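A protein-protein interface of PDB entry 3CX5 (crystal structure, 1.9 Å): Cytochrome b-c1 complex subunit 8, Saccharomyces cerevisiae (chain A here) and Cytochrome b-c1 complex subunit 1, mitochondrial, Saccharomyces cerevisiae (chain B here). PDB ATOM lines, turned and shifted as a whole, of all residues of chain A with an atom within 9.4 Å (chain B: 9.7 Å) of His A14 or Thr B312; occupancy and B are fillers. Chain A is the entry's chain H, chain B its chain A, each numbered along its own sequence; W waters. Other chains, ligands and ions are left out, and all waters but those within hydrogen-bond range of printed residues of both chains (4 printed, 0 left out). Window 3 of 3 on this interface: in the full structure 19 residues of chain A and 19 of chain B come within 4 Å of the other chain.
Printed residues of chain B within 4 Å of His A14: Thr B312 and Glu B414. Of chain A, only Trp A12 (3.7 Å) and His A14 (3.6 Å) come within 4 Å of Thr B312. No residue of chain B comes within 4 Å of Gly A10. Gly A13 touches two residues of chain B. Of the printed residues of chain B, Met A15 touches Glu B414. Of the printed residues of chain A, Glu B414 touches Trp A11 (3.6 Å), Trp A12 (3.6 Å), Gly A13 (2.9 Å), His A14 (3.0 Å) and Met A15 (2.8 Å). Printed residues of chain A within 4 Å of Asp B228: Pro A18 (3.9 Å) and Lys A19 (3.7 Å). The nearest residue of chain B that does not touch His A14 is Val B311 (5.8 Å). The nearest printed residue of chain B that does not touch Trp A11 is Thr B312 (6.0 Å).
OD2 of Asp B228 is in salt-bridge range of NH2 of Arg B226, at 2.8 Å. The guanidinium group (NH2) of Arg B226 lies within salt-bridge range of the side-chain carboxylate (OE2) of Glu B414 (3.4 Å). The backbone carbonyl oxygen (O) of Met A15 sits at hydrogen-bond distance from the backbone NH (N) of Gly A10, 2.9 Å away.
The backbone NH of Gly A13 lies within hydrogen-bond range of the side-chain carboxylate of Glu B414, at 2.9 Å. The side-chain carboxylate (OE1) of Glu B414 is in hydrogen-bond range of the backbone NH (N) of His A14 (3.0 Å). The side-chain carboxylate (OE1) of Glu B414 is in hydrogen-bond range of the backbone NH (N) of Met A15 (2.8 Å).
Water W4 bridges the backbone carbonyl oxygen of Trp A12 (2.7 Å) and the backbone carbonyl oxygen of Thr B312 (2.8 Å). Water W3 bridges the side-chain carboxylate (OE2) of Glu B414 (2.7 Å) and the backbone NH (N) of Gly A17 (2.9 Å). Water W2 lies within hydrogen-bond range of the backbone carbonyl oxygen (O) of Gly A13 (2.7 Å) and the side-chain amide nitrogen (NE2) of Gln B412 (2.7 Å). Water W1 bridges the side-chain carboxylate of Asp B228 and the backbone carbonyl oxygen of Pro A18.
Trp A11 touches Glu B414 (O to OE1, 3.6 Å). Trp A12 touches Thr B312 (O to CA, 3.7 Å). Glu B414 touches Trp A12. Gly A13 touches Val B311 (CA to O, 3.5 Å). His A14 touches Thr B312. Pro A18 touches Asp B228. Lys A19 touches Asp B228.
Printed residues of chain A that touch a printed residue of chain B: Trp A11, Trp A12, Gly A13, His A14, Met A15, Pro A18 and Lys A19. Among the printed residues, 10 pairs touch across the chains.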
ATOM      1  N   THR A   7      15.831 -23.501  25.185  1.00  0.00           N
ATOM      2  CA  THR A   7      16.696 -24.620  24.824  1.00  0.00           C
ATOM      3  C   THR A   7      16.538 -24.865  23.329  1.00  0.00           C
ATOM      4  O   THR A   7      15.881 -24.088  22.638  1.00  0.00           O
ATOM      5  CB  THR A   7      16.298 -25.906  25.569  1.00  0.00           C
ATOM      6  OG1 THR A   7      14.970 -26.286  25.185  1.00  0.00           O
ATOM      7  CG2 THR A   7      16.345 -25.687  27.077  1.00  0.00           C
ATOM      8  N   TYR A   8      17.101 -25.966  22.840  1.00  0.00           N
ATOM      9  CA  TYR A   8      17.009 -26.294  21.424  1.00  0.00           C
ATOM     10  C   TYR A   8      15.975 -27.370  21.078  1.00  0.00           C
ATOM     11  O   TYR A   8      15.924 -27.835  19.941  1.00  0.00           O
ATOM     12  CB  TYR A   8      18.394 -26.638  20.869  1.00  0.00           C
ATOM     13  CG  TYR A   8      19.324 -25.442  20.854  1.00  0.00           C
ATOM     14  CD1 TYR A   8      20.259 -25.239  21.876  1.00  0.00           C
ATOM     15  CD2 TYR A   8      19.243 -24.490  19.835  1.00  0.00           C
ATOM     16  CE1 TYR A   8      21.093 -24.105  21.880  1.00  0.00           C
ATOM     17  CE2 TYR A   8      20.068 -23.360  19.828  1.00  0.00           C
ATOM     18  CZ  TYR A   8      20.987 -23.175  20.849  1.00  0.00           C
ATOM     19  OH  TYR A   8      21.801 -22.062  20.824  1.00  0.00           O
ATOM     20  N   MET A   9      15.171 -27.776  22.060  1.00  0.00           N
ATOM     21  CA  MET A   9      14.105 -28.755  21.833  1.00  0.00           C
ATOM     22  C   MET A   9      12.849 -28.289  22.563  1.00  0.00           C
ATOM     23  O   MET A   9      12.927 -27.831  23.701  1.00  0.00           O
ATOM     24  CB  MET A   9      14.484 -30.159  22.329  1.00  0.00           C
ATOM     25  CG  MET A   9      13.403 -31.205  22.034  1.00  0.00           C
ATOM     26  SD  MET A   9      13.697 -32.861  22.680  1.00  0.00           S
ATOM     27  CE  MET A   9      13.046 -32.736  24.359  1.00  0.00           C
ATOM     28  N   GLY A  10      11.705 -28.367  21.888  1.00  0.00           N
ATOM     29  CA  GLY A  10      10.445 -27.977  22.498  1.00  0.00           C
ATOM     30  C   GLY A  10       9.654 -29.225  22.848  1.00  0.00           C
ATOM     31  O   GLY A  10      10.177 -30.130  23.496  1.00  0.00           O
ATOM     32  N   TRP A  11       8.398 -29.284  22.407  1.00  0.00           N
ATOM     33  CA  TRP A  11       7.538 -30.442  22.660  1.00  0.00           C
ATOM     34  C   TRP A  11       6.601 -30.566  21.465  1.00  0.00           C
ATOM     35  O   TRP A  11       6.672 -29.755  20.547  1.00  0.00           O
ATOM     36  CB  TRP A  11       6.739 -30.244  23.954  1.00  0.00           C
ATOM     37  CG  TRP A  11       6.347 -31.525  24.647  1.00  0.00           C
ATOM     38  CD1 TRP A  11       5.089 -32.055  24.738  1.00  0.00           C
ATOM     39  CD2 TRP A  11       7.206 -32.404  25.394  1.00  0.00           C
ATOM     40  NE1 TRP A  11       5.108 -33.199  25.498  1.00  0.00           N
ATOM     41  CE2 TRP A  11       6.392 -33.439  25.914  1.00  0.00           C
ATOM     42  CE3 TRP A  11       8.583 -32.413  25.680  1.00  0.00           C
ATOM     43  CZ2 TRP A  11       6.908 -34.477  26.705  1.00  0.00           C
ATOM     44  CZ3 TRP A  11       9.097 -33.446  26.472  1.00  0.00           C
ATOM     45  CH2 TRP A  11       8.255 -34.464  26.974  1.00  0.00           C
ATOM     46  N   TRP A  12       5.724 -31.570  21.477  1.00  0.00           N
ATOM     47  CA  TRP A  12       4.782 -31.797  20.379  1.00  0.00           C
ATOM     48  C   TRP A  12       3.981 -30.532  20.035  1.00  0.00           C
ATOM     49  O   TRP A  12       3.352 -29.919  20.907  1.00  0.00           O
ATOM     50  CB  TRP A  12       3.844 -32.957  20.723  1.00  0.00           C
ATOM     51  CG  TRP A  12       4.551 -34.258  21.038  1.00  0.00           C
ATOM     52  CD1 TRP A  12       4.698 -34.830  22.267  1.00  0.00           C
ATOM     53  CD2 TRP A  12       5.208 -35.138  20.108  1.00  0.00           C
ATOM     54  NE1 TRP A  12       5.405 -36.003  22.166  1.00  0.00           N
ATOM     55  CE2 TRP A  12       5.730 -36.216  20.853  1.00  0.00           C
ATOM     56  CE3 TRP A  12       5.409 -35.113  18.722  1.00  0.00           C
ATOM     57  CZ2 TRP A  12       6.445 -37.261  20.263  1.00  0.00           C
ATOM     58  CZ3 TRP A  12       6.121 -36.157  18.131  1.00  0.00           C
ATOM     59  CH2 TRP A  12       6.630 -37.215  18.904  1.00  0.00           C
ATOM     60  N   GLY A  13       4.023 -30.141  18.763  1.00  0.00           N
ATOM     61  CA  GLY A  13       3.329 -28.944  18.321  1.00  0.00           C
ATOM     62  C   GLY A  13       4.259 -27.748  18.172  1.00  0.00           C
ATOM     63  O   GLY A  13       3.946 -26.807  17.443  1.00  0.00           O
ATOM     64  N   HIS A  14       5.389 -27.777  18.877  1.00  0.00           N
ATOM     65  CA  HIS A  14       6.394 -26.704  18.833  1.00  0.00           C
ATOM     66  C   HIS A  14       7.762 -27.315  19.164  1.00  0.00           C
ATOM     67  O   HIS A  14       8.435 -26.903  20.111  1.00  0.00           O
ATOM     68  CB  HIS A  14       6.036 -25.595  19.843  1.00  0.00           C
ATOM     69  CG  HIS A  14       5.922 -26.069  21.266  1.00  0.00           C
ATOM     70  ND1 HIS A  14       6.867 -25.771  22.228  1.00  0.00           N
ATOM     71  CD2 HIS A  14       4.973 -26.807  21.892  1.00  0.00           C
ATOM     72  CE1 HIS A  14       6.500 -26.302  23.383  1.00  0.00           C
ATOM     73  NE2 HIS A  14       5.355 -26.936  23.206  1.00  0.00           N
ATOM     74  N   MET A  15       8.178 -28.299  18.369  1.00  0.00           N
ATOM     75  CA  MET A  15       9.433 -29.002  18.604  1.00  0.00           C
ATOM     76  C   MET A  15      10.689 -28.146  18.427  1.00  0.00           C
ATOM     77  O   MET A  15      11.741 -28.483  18.957  1.00  0.00           O
ATOM     78  CB  MET A  15       9.512 -30.270  17.737  1.00  0.00           C
ATOM     79  CG  MET A  15      10.382 -31.405  18.307  1.00  0.00           C
ATOM     80  SD  MET A  15       9.707 -32.196  19.812  1.00  0.00           S
ATOM     81  CE  MET A  15       8.175 -32.970  19.181  1.00  0.00           C
ATOM     82  N   GLY A  16      10.579 -27.041  17.699  1.00  0.00           N
ATOM     83  CA  GLY A  16      11.735 -26.177  17.516  1.00  0.00           C
ATOM     84  C   GLY A  16      12.497 -26.369  16.217  1.00  0.00           C
ATOM     85  O   GLY A  16      13.586 -25.806  16.043  1.00  0.00           O
ATOM     86  N   GLY A  17      11.942 -27.180  15.315  1.00  0.00           N
ATOM     87  CA  GLY A  17      12.581 -27.403  14.031  1.00  0.00           C
ATOM     88  C   GLY A  17      12.112 -26.368  13.020  1.00  0.00           C
ATOM     89  O   GLY A  17      11.364 -25.457  13.373  1.00  0.00           O
ATOM     90  N   PRO A  18      12.567 -26.448  11.763  1.00  0.00           N
ATOM     91  CA  PRO A  18      12.119 -25.462  10.777  1.00  0.00           C
ATOM     92  C   PRO A  18      10.699 -25.775  10.312  1.00  0.00           C
ATOM     93  O   PRO A  18      10.183 -26.866  10.559  1.00  0.00           O
ATOM     94  CB  PRO A  18      13.136 -25.626   9.646  1.00  0.00           C
ATOM     95  CG  PRO A  18      13.495 -27.071   9.718  1.00  0.00           C
ATOM     96  CD  PRO A  18      13.607 -27.331  11.205  1.00  0.00           C
ATOM     97  N   LYS A  19      10.055 -24.801   9.678  1.00  0.00           N
ATOM     98  CA  LYS A  19       8.710 -25.001   9.165  1.00  0.00           C
ATOM     99  C   LYS A  19       8.792 -26.052   8.063  1.00  0.00           C
ATOM    100  O   LYS A  19       9.675 -26.001   7.208  1.00  0.00           O
ATOM    101  CB  LYS A  19       8.135 -23.691   8.623  1.00  0.00           C
ATOM    102  CG  LYS A  19       7.907 -22.640   9.692  1.00  0.00           C
ATOM    103  CD  LYS A  19       6.846 -21.634   9.266  1.00  0.00           C
ATOM    104  CE  LYS A  19       6.662 -20.539  10.313  1.00  0.00           C
ATOM    105  NZ  LYS A  19       6.425 -21.105  11.670  1.00  0.00           N
ATOM    106  N   ARG B 226       1.899 -32.624   6.070  1.00  0.00           N
ATOM    107  CA  ARG B 226       2.253 -31.532   6.960  1.00  0.00           C
ATOM    108  C   ARG B 226       2.556 -30.229   6.233  1.00  0.00           C
ATOM    109  O   ARG B 226       3.246 -30.217   5.217  1.00  0.00           O
ATOM    110  CB  ARG B 226       3.448 -31.881   7.851  1.00  0.00           C
ATOM    111  CG  ARG B 226       3.429 -31.050   9.125  1.00  0.00           C
ATOM    112  CD  ARG B 226       4.779 -30.585   9.592  1.00  0.00           C
ATOM    113  NE  ARG B 226       5.439 -31.530  10.472  1.00  0.00           N
ATOM    114  CZ  ARG B 226       6.253 -31.193  11.473  1.00  0.00           C
ATOM    115  NH1 ARG B 226       6.816 -32.146  12.197  1.00  0.00           N
ATOM    116  NH2 ARG B 226       6.482 -29.918  11.777  1.00  0.00           N
ATOM    117  N   ASP B 228       3.375 -26.524   7.950  1.00  0.00           N
ATOM    118  CA  ASP B 228       3.491 -25.622   9.089  1.00  0.00           C
ATOM    119  C   ASP B 228       3.128 -24.165   8.815  1.00  0.00           C
ATOM    120  O   ASP B 228       3.072 -23.356   9.750  1.00  0.00           O
ATOM    121  CB  ASP B 228       4.885 -25.728   9.721  1.00  0.00           C
ATOM    122  CG  ASP B 228       5.157 -27.112  10.304  1.00  0.00           C
ATOM    123  OD1 ASP B 228       4.191 -27.792  10.728  1.00  0.00           O
ATOM    124  OD2 ASP B 228       6.339 -27.526  10.343  1.00  0.00           O
ATOM    125  N   PRO B 231      -2.674 -22.175   9.334  1.00  0.00           N
ATOM    126  CA  PRO B 231      -3.108 -21.828  10.695  1.00  0.00           C
ATOM    127  C   PRO B 231      -3.732 -22.912  11.570  1.00  0.00           C
ATOM    128  O   PRO B 231      -3.863 -22.726  12.781  1.00  0.00           O
ATOM    129  CB  PRO B 231      -4.073 -20.671  10.453  1.00  0.00           C
ATOM    130  CG  PRO B 231      -4.689 -21.022   9.137  1.00  0.00           C
ATOM    131  CD  PRO B 231      -3.518 -21.509   8.323  1.00  0.00           C
ATOM    132  N   LYS B 232      -4.123 -24.035  10.977  1.00  0.00           N
ATOM    133  CA  LYS B 232      -4.738 -25.109  11.752  1.00  0.00           C
ATOM    134  C   LYS B 232      -4.181 -26.467  11.368  1.00  0.00           C
ATOM    135  O   LYS B 232      -3.282 -26.584  10.537  1.00  0.00           O
ATOM    136  CB  LYS B 232      -6.257 -25.167  11.505  1.00  0.00           C
ATOM    137  CG  LYS B 232      -7.012 -23.846  11.551  1.00  0.00           C
ATOM    138  CD  LYS B 232      -8.521 -24.085  11.496  1.00  0.00           C
ATOM    139  CE  LYS B 232      -9.295 -22.765  11.538  1.00  0.00           C
ATOM    140  NZ  LYS B 232     -10.701 -22.952  12.017  1.00  0.00           N
ATOM    141  N   ALA B 233      -4.730 -27.485  12.022  1.00  0.00           N
ATOM    142  CA  ALA B 233      -4.421 -28.871  11.755  1.00  0.00           C
ATOM    143  C   ALA B 233      -5.793 -29.406  11.368  1.00  0.00           C
ATOM    144  O   ALA B 233      -6.786 -29.116  12.046  1.00  0.00           O
ATOM    145  CB  ALA B 233      -3.913 -29.576  13.009  1.00  0.00           C
ATOM    146  N   TYR B 283     -10.167 -27.287  27.679  1.00  0.00           N
ATOM    147  CA  TYR B 283      -8.984 -26.642  27.112  1.00  0.00           C
ATOM    148  C   TYR B 283      -9.184 -26.357  25.621  1.00  0.00           C
ATOM    149  O   TYR B 283      -8.221 -26.122  24.895  1.00  0.00           O
ATOM    150  CB  TYR B 283      -7.745 -27.526  27.310  1.00  0.00           C
ATOM    151  CG  TYR B 283      -7.319 -27.690  28.751  1.00  0.00           C
ATOM    152  CD1 TYR B 283      -7.878 -28.679  29.557  1.00  0.00           C
ATOM    153  CD2 TYR B 283      -6.357 -26.847  29.313  1.00  0.00           C
ATOM    154  CE1 TYR B 283      -7.495 -28.828  30.893  1.00  0.00           C
ATOM    155  CE2 TYR B 283      -5.962 -26.986  30.650  1.00  0.00           C
ATOM    156  CZ  TYR B 283      -6.538 -27.976  31.432  1.00  0.00           C
ATOM    157  OH  TYR B 283      -6.165 -28.104  32.751  1.00  0.00           O
ATOM    158  N   GLN B 284     -10.444 -26.364  25.189  1.00  0.00           N
ATOM    159  CA  GLN B 284     -10.845 -26.142  23.797  1.00  0.00           C
ATOM    160  C   GLN B 284      -9.932 -26.831  22.788  1.00  0.00           C
ATOM    161  O   GLN B 284      -9.145 -26.198  22.078  1.00  0.00           O
ATOM    162  CB  GLN B 284     -11.016 -24.655  23.474  1.00  0.00           C
ATOM    163  CG  GLN B 284     -11.981 -24.414  22.283  1.00  0.00           C
ATOM    164  CD  GLN B 284     -13.351 -25.077  22.475  1.00  0.00           C
ATOM    165  OE1 GLN B 284     -14.151 -24.660  23.322  1.00  0.00           O
ATOM    166  NE2 GLN B 284     -13.614 -26.121  21.699  1.00  0.00           N
ATOM    167  N   LEU B 285     -10.085 -28.145  22.728  1.00  0.00           N
ATOM    168  CA  LEU B 285      -9.298 -29.010  21.865  1.00  0.00           C
ATOM    169  C   LEU B 285      -9.510 -28.852  20.358  1.00  0.00           C
ATOM    170  O   LEU B 285      -8.642 -29.234  19.574  1.00  0.00           O
ATOM    171  CB  LEU B 285      -9.502 -30.465  22.306  1.00  0.00           C
ATOM    172  CG  LEU B 285      -8.547 -31.032  23.371  1.00  0.00           C
ATOM    173  CD1 LEU B 285      -7.913 -29.948  24.247  1.00  0.00           C
ATOM    174  CD2 LEU B 285      -9.265 -32.065  24.199  1.00  0.00           C
ATOM    175  N   THR B 308      -8.484 -27.864  14.088  1.00  0.00           N
ATOM    176  CA  THR B 308      -8.079 -27.273  15.353  1.00  0.00           C
ATOM    177  C   THR B 308      -6.889 -26.331  15.280  1.00  0.00           C
ATOM    178  O   THR B 308      -5.960 -26.526  14.496  1.00  0.00           O
ATOM    179  CB  THR B 308      -7.770 -28.385  16.406  1.00  0.00           C
ATOM    180  OG1 THR B 308      -7.335 -27.786  17.632  1.00  0.00           O
ATOM    181  CG2 THR B 308      -6.696 -29.334  15.900  1.00  0.00           C
ATOM    182  N   ARG B 309      -6.933 -25.311  16.126  1.00  0.00           N
ATOM    183  CA  ARG B 309      -5.851 -24.337  16.248  1.00  0.00           C
ATOM    184  C   ARG B 309      -5.059 -24.688  17.511  1.00  0.00           C
ATOM    185  O   ARG B 309      -4.029 -24.085  17.791  1.00  0.00           O
ATOM    186  CB  ARG B 309      -6.412 -22.914  16.344  1.00  0.00           C
ATOM    187  CG  ARG B 309      -6.880 -22.339  15.001  1.00  0.00           C
ATOM    188  CD  ARG B 309      -8.147 -21.502  15.146  1.00  0.00           C
ATOM    189  NE  ARG B 309      -7.994 -20.421  16.108  1.00  0.00           N
ATOM    190  CZ  ARG B 309      -8.794 -20.202  17.149  1.00  0.00           C
ATOM    191  NH1 ARG B 309      -8.543 -19.176  17.949  1.00  0.00           N
ATOM    192  NH2 ARG B 309      -9.830 -20.996  17.405  1.00  0.00           N
ATOM    193  N   ASN B 310      -5.551 -25.662  18.277  1.00  0.00           N
ATOM    194  CA  ASN B 310      -4.864 -26.105  19.495  1.00  0.00           C
ATOM    195  C   ASN B 310      -3.858 -27.187  19.071  1.00  0.00           C
ATOM    196  O   ASN B 310      -4.024 -28.375  19.359  1.00  0.00           O
ATOM    197  CB  ASN B 310      -5.871 -26.661  20.514  1.00  0.00           C
ATOM    198  CG  ASN B 310      -5.306 -26.731  21.936  1.00  0.00           C
ATOM    199  OD1 ASN B 310      -6.060 -26.774  22.916  1.00  0.00           O
ATOM    200  ND2 ASN B 310      -3.983 -26.714  22.053  1.00  0.00           N
ATOM    201  N   VAL B 311      -2.785 -26.734  18.431  1.00  0.00           N
ATOM    202  CA  VAL B 311      -1.747 -27.600  17.896  1.00  0.00           C
ATOM    203  C   VAL B 311      -0.866 -28.354  18.888  1.00  0.00           C
ATOM    204  O   VAL B 311      -0.161 -29.277  18.496  1.00  0.00           O
ATOM    205  CB  VAL B 311      -0.856 -26.834  16.880  1.00  0.00           C
ATOM    206  CG1 VAL B 311      -1.719 -26.260  15.753  1.00  0.00           C
ATOM    207  CG2 VAL B 311      -0.079 -25.729  17.579  1.00  0.00           C
ATOM    208  N   THR B 312      -0.891 -27.967  20.161  1.00  0.00           N
ATOM    209  CA  THR B 312      -0.084 -28.651  21.169  1.00  0.00           C
ATOM    210  C   THR B 312      -0.889 -29.703  21.933  1.00  0.00           C
ATOM    211  O   THR B 312      -0.332 -30.454  22.737  1.00  0.00           O
ATOM    212  CB  THR B 312       0.519 -27.660  22.184  1.00  0.00           C
ATOM    213  OG1 THR B 312      -0.536 -26.958  22.853  1.00  0.00           O
ATOM    214  CG2 THR B 312       1.426 -26.649  21.480  1.00  0.00           C
ATOM    215  N   MET B 313      -2.190 -29.785  21.661  1.00  0.00           N
ATOM    216  CA  MET B 313      -3.038 -30.744  22.364  1.00  0.00           C
ATOM    217  C   MET B 313      -3.815 -31.681  21.456  1.00  0.00           C
ATOM    218  O   MET B 313      -4.842 -32.242  21.853  1.00  0.00           O
ATOM    219  CB  MET B 313      -3.978 -30.018  23.341  1.00  0.00           C
ATOM    220  CG  MET B 313      -3.248 -29.268  24.457  1.00  0.00           C
ATOM    221  SD  MET B 313      -4.334 -28.487  25.681  1.00  0.00           S
ATOM    222  CE  MET B 313      -4.611 -29.854  26.815  1.00  0.00           C
ATOM    223  N   ILE B 314      -3.304 -31.867  20.242  1.00  0.00           N
ATOM    224  CA  ILE B 314      -3.922 -32.757  19.263  1.00  0.00           C
ATOM    225  C   ILE B 314      -4.010 -34.167  19.825  1.00  0.00           C
ATOM    226  O   ILE B 314      -5.015 -34.860  19.621  1.00  0.00           O
ATOM    227  CB  ILE B 314      -3.130 -32.757  17.937  1.00  0.00           C
ATOM    228  CG1 ILE B 314      -3.261 -31.387  17.271  1.00  0.00           C
ATOM    229  CG2 ILE B 314      -3.635 -33.855  16.998  1.00  0.00           C
ATOM    230  CD1 ILE B 314      -2.459 -31.234  16.004  1.00  0.00           C
ATOM    231  N   ASP B 315      -2.975 -34.583  20.558  1.00  0.00           N
ATOM    232  CA  ASP B 315      -2.973 -35.916  21.157  1.00  0.00           C
ATOM    233  C   ASP B 315      -4.174 -36.118  22.092  1.00  0.00           C
ATOM    234  O   ASP B 315      -4.743 -37.201  22.131  1.00  0.00           O
ATOM    235  CB  ASP B 315      -1.648 -36.212  21.878  1.00  0.00           C
ATOM    236  CG  ASP B 315      -1.436 -35.352  23.120  1.00  0.00           C
ATOM    237  OD1 ASP B 315      -1.488 -34.103  23.014  1.00  0.00           O
ATOM    238  OD2 ASP B 315      -1.218 -35.927  24.209  1.00  0.00           O
ATOM    239  N   ASP B 316      -4.572 -35.078  22.824  1.00  0.00           N
ATOM    240  CA  ASP B 316      -5.732 -35.191  23.708  1.00  0.00           C
ATOM    241  C   ASP B 316      -7.036 -35.259  22.899  1.00  0.00           C
ATOM    242  O   ASP B 316      -7.945 -36.013  23.250  1.00  0.00           O
ATOM    243  CB  ASP B 316      -5.796 -34.020  24.698  1.00  0.00           C
ATOM    244  CG  ASP B 316      -4.661 -34.047  25.709  1.00  0.00           C
ATOM    245  OD1 ASP B 316      -3.849 -33.096  25.709  1.00  0.00           O
ATOM    246  OD2 ASP B 316      -4.578 -35.022  26.493  1.00  0.00           O
ATOM    247  N   LEU B 317      -7.110 -34.486  21.817  1.00  0.00           N
ATOM    248  CA  LEU B 317      -8.293 -34.464  20.949  1.00  0.00           C
ATOM    249  C   LEU B 317      -8.570 -35.875  20.446  1.00  0.00           C
ATOM    250  O   LEU B 317      -9.676 -36.401  20.605  1.00  0.00           O
ATOM    251  CB  LEU B 317      -8.046 -33.571  19.729  1.00  0.00           C
ATOM    252  CG  LEU B 317      -9.144 -32.716  19.085  1.00  0.00           C
ATOM    253  CD1 LEU B 317      -8.823 -32.554  17.608  1.00  0.00           C
ATOM    254  CD2 LEU B 317     -10.541 -33.284  19.280  1.00  0.00           C
ATOM    255  N   GLN B 412      -0.674 -27.963  10.586  1.00  0.00           N
ATOM    256  CA  GLN B 412       0.208 -28.119  11.737  1.00  0.00           C
ATOM    257  C   GLN B 412      -0.079 -29.394  12.515  1.00  0.00           C
ATOM    258  O   GLN B 412      -0.570 -29.354  13.646  1.00  0.00           O
ATOM    259  CB  GLN B 412       0.102 -26.888  12.642  1.00  0.00           C
ATOM    260  CG  GLN B 412       0.742 -25.641  12.039  1.00  0.00           C
ATOM    261  CD  GLN B 412       0.671 -24.436  12.967  1.00  0.00           C
ATOM    262  OE1 GLN B 412       0.155 -23.375  12.598  1.00  0.00           O
ATOM    263  NE2 GLN B 412       1.172 -24.601  14.181  1.00  0.00           N
ATOM    264  N   ILE B 413       0.269 -30.523  11.903  1.00  0.00           N
ATOM    265  CA  ILE B 413       0.034 -31.836  12.483  1.00  0.00           C
ATOM    266  C   ILE B 413       1.233 -32.481  13.183  1.00  0.00           C
ATOM    267  O   ILE B 413       1.254 -33.693  13.395  1.00  0.00           O
ATOM    268  CB  ILE B 413      -0.536 -32.816  11.426  1.00  0.00           C
ATOM    269  CG1 ILE B 413       0.391 -32.885  10.206  1.00  0.00           C
ATOM    270  CG2 ILE B 413      -1.941 -32.393  11.029  1.00  0.00           C
ATOM    271  CD1 ILE B 413      -0.003 -33.937   9.178  1.00  0.00           C
ATOM    272  N   GLU B 414       2.235 -31.682  13.542  1.00  0.00           N
ATOM    273  CA  GLU B 414       3.390 -32.221  14.252  1.00  0.00           C
ATOM    274  C   GLU B 414       2.910 -32.945  15.517  1.00  0.00           C
ATOM    275  O   GLU B 414       3.429 -34.003  15.872  1.00  0.00           O
ATOM    276  CB  GLU B 414       4.360 -31.101  14.647  1.00  0.00           C
ATOM    277  CG  GLU B 414       5.564 -31.597  15.456  1.00  0.00           C
ATOM    278  CD  GLU B 414       6.493 -30.475  15.878  1.00  0.00           C
ATOM    279  OE1 GLU B 414       6.324 -29.948  17.003  1.00  0.00           O
ATOM    280  OE2 GLU B 414       7.396 -30.130  15.086  1.00  0.00           O
ATOM    281  N   GLY B 415       1.897 -32.370  16.162  1.00  0.00           N
ATOM    282  CA  GLY B 415       1.333 -32.924  17.382  1.00  0.00           C
ATOM    283  C   GLY B 415       0.515 -34.194  17.231  1.00  0.00           C
ATOM    284  O   GLY B 415       0.115 -34.786  18.234  1.00  0.00           O
ATOM    285  N   LEU B 416       0.211 -34.587  15.994  1.00  0.00           N
ATOM    286  CA  LEU B 416      -0.535 -35.827  15.761  1.00  0.00           C
ATOM    287  C   LEU B 416       0.514 -36.932  15.913  1.00  0.00           C
ATOM    288  O   LEU B 416       1.476 -36.986  15.148  1.00  0.00           O
ATOM    289  CB  LEU B 416      -1.133 -35.852  14.350  1.00  0.00           C
ATOM    290  CG  LEU B 416      -1.940 -37.097  13.940  1.00  0.00           C
ATOM    291  CD1 LEU B 416      -3.191 -37.212  14.789  1.00  0.00           C
ATOM    292  CD2 LEU B 416      -2.304 -37.020  12.455  1.00  0.00           C
ATOM    293  N   LEU B 417       0.362 -37.769  16.934  1.00  0.00           N
ATOM    294  CA  LEU B 417       1.317 -38.847  17.193  1.00  0.00           C
ATOM    295  C   LEU B 417       1.370 -39.902  16.084  1.00  0.00           C
ATOM    296  O   LEU B 417       0.599 -39.857  15.129  1.00  0.00           O
ATOM    297  CB  LEU B 417       1.019 -39.503  18.547  1.00  0.00           C
ATOM    298  CG  LEU B 417       1.658 -38.910  19.814  1.00  0.00           C
ATOM    299  CD1 LEU B 417       1.891 -37.418  19.693  1.00  0.00           C
ATOM    300  CD2 LEU B 417       0.804 -39.230  21.031  1.00  0.00           C
HETATM  301  O   HOH W   1       7.858 -26.359  12.920  1.00  0.00           O
HETATM  302  O   HOH W   2       2.740 -26.699  14.993  1.00  0.00           O
HETATM  303  O   HOH W   3       9.343 -28.288  14.664  1.00  0.00           O
HETATM  304  O   HOH W   4       2.446 -30.652  23.309  1.00  0.00           O
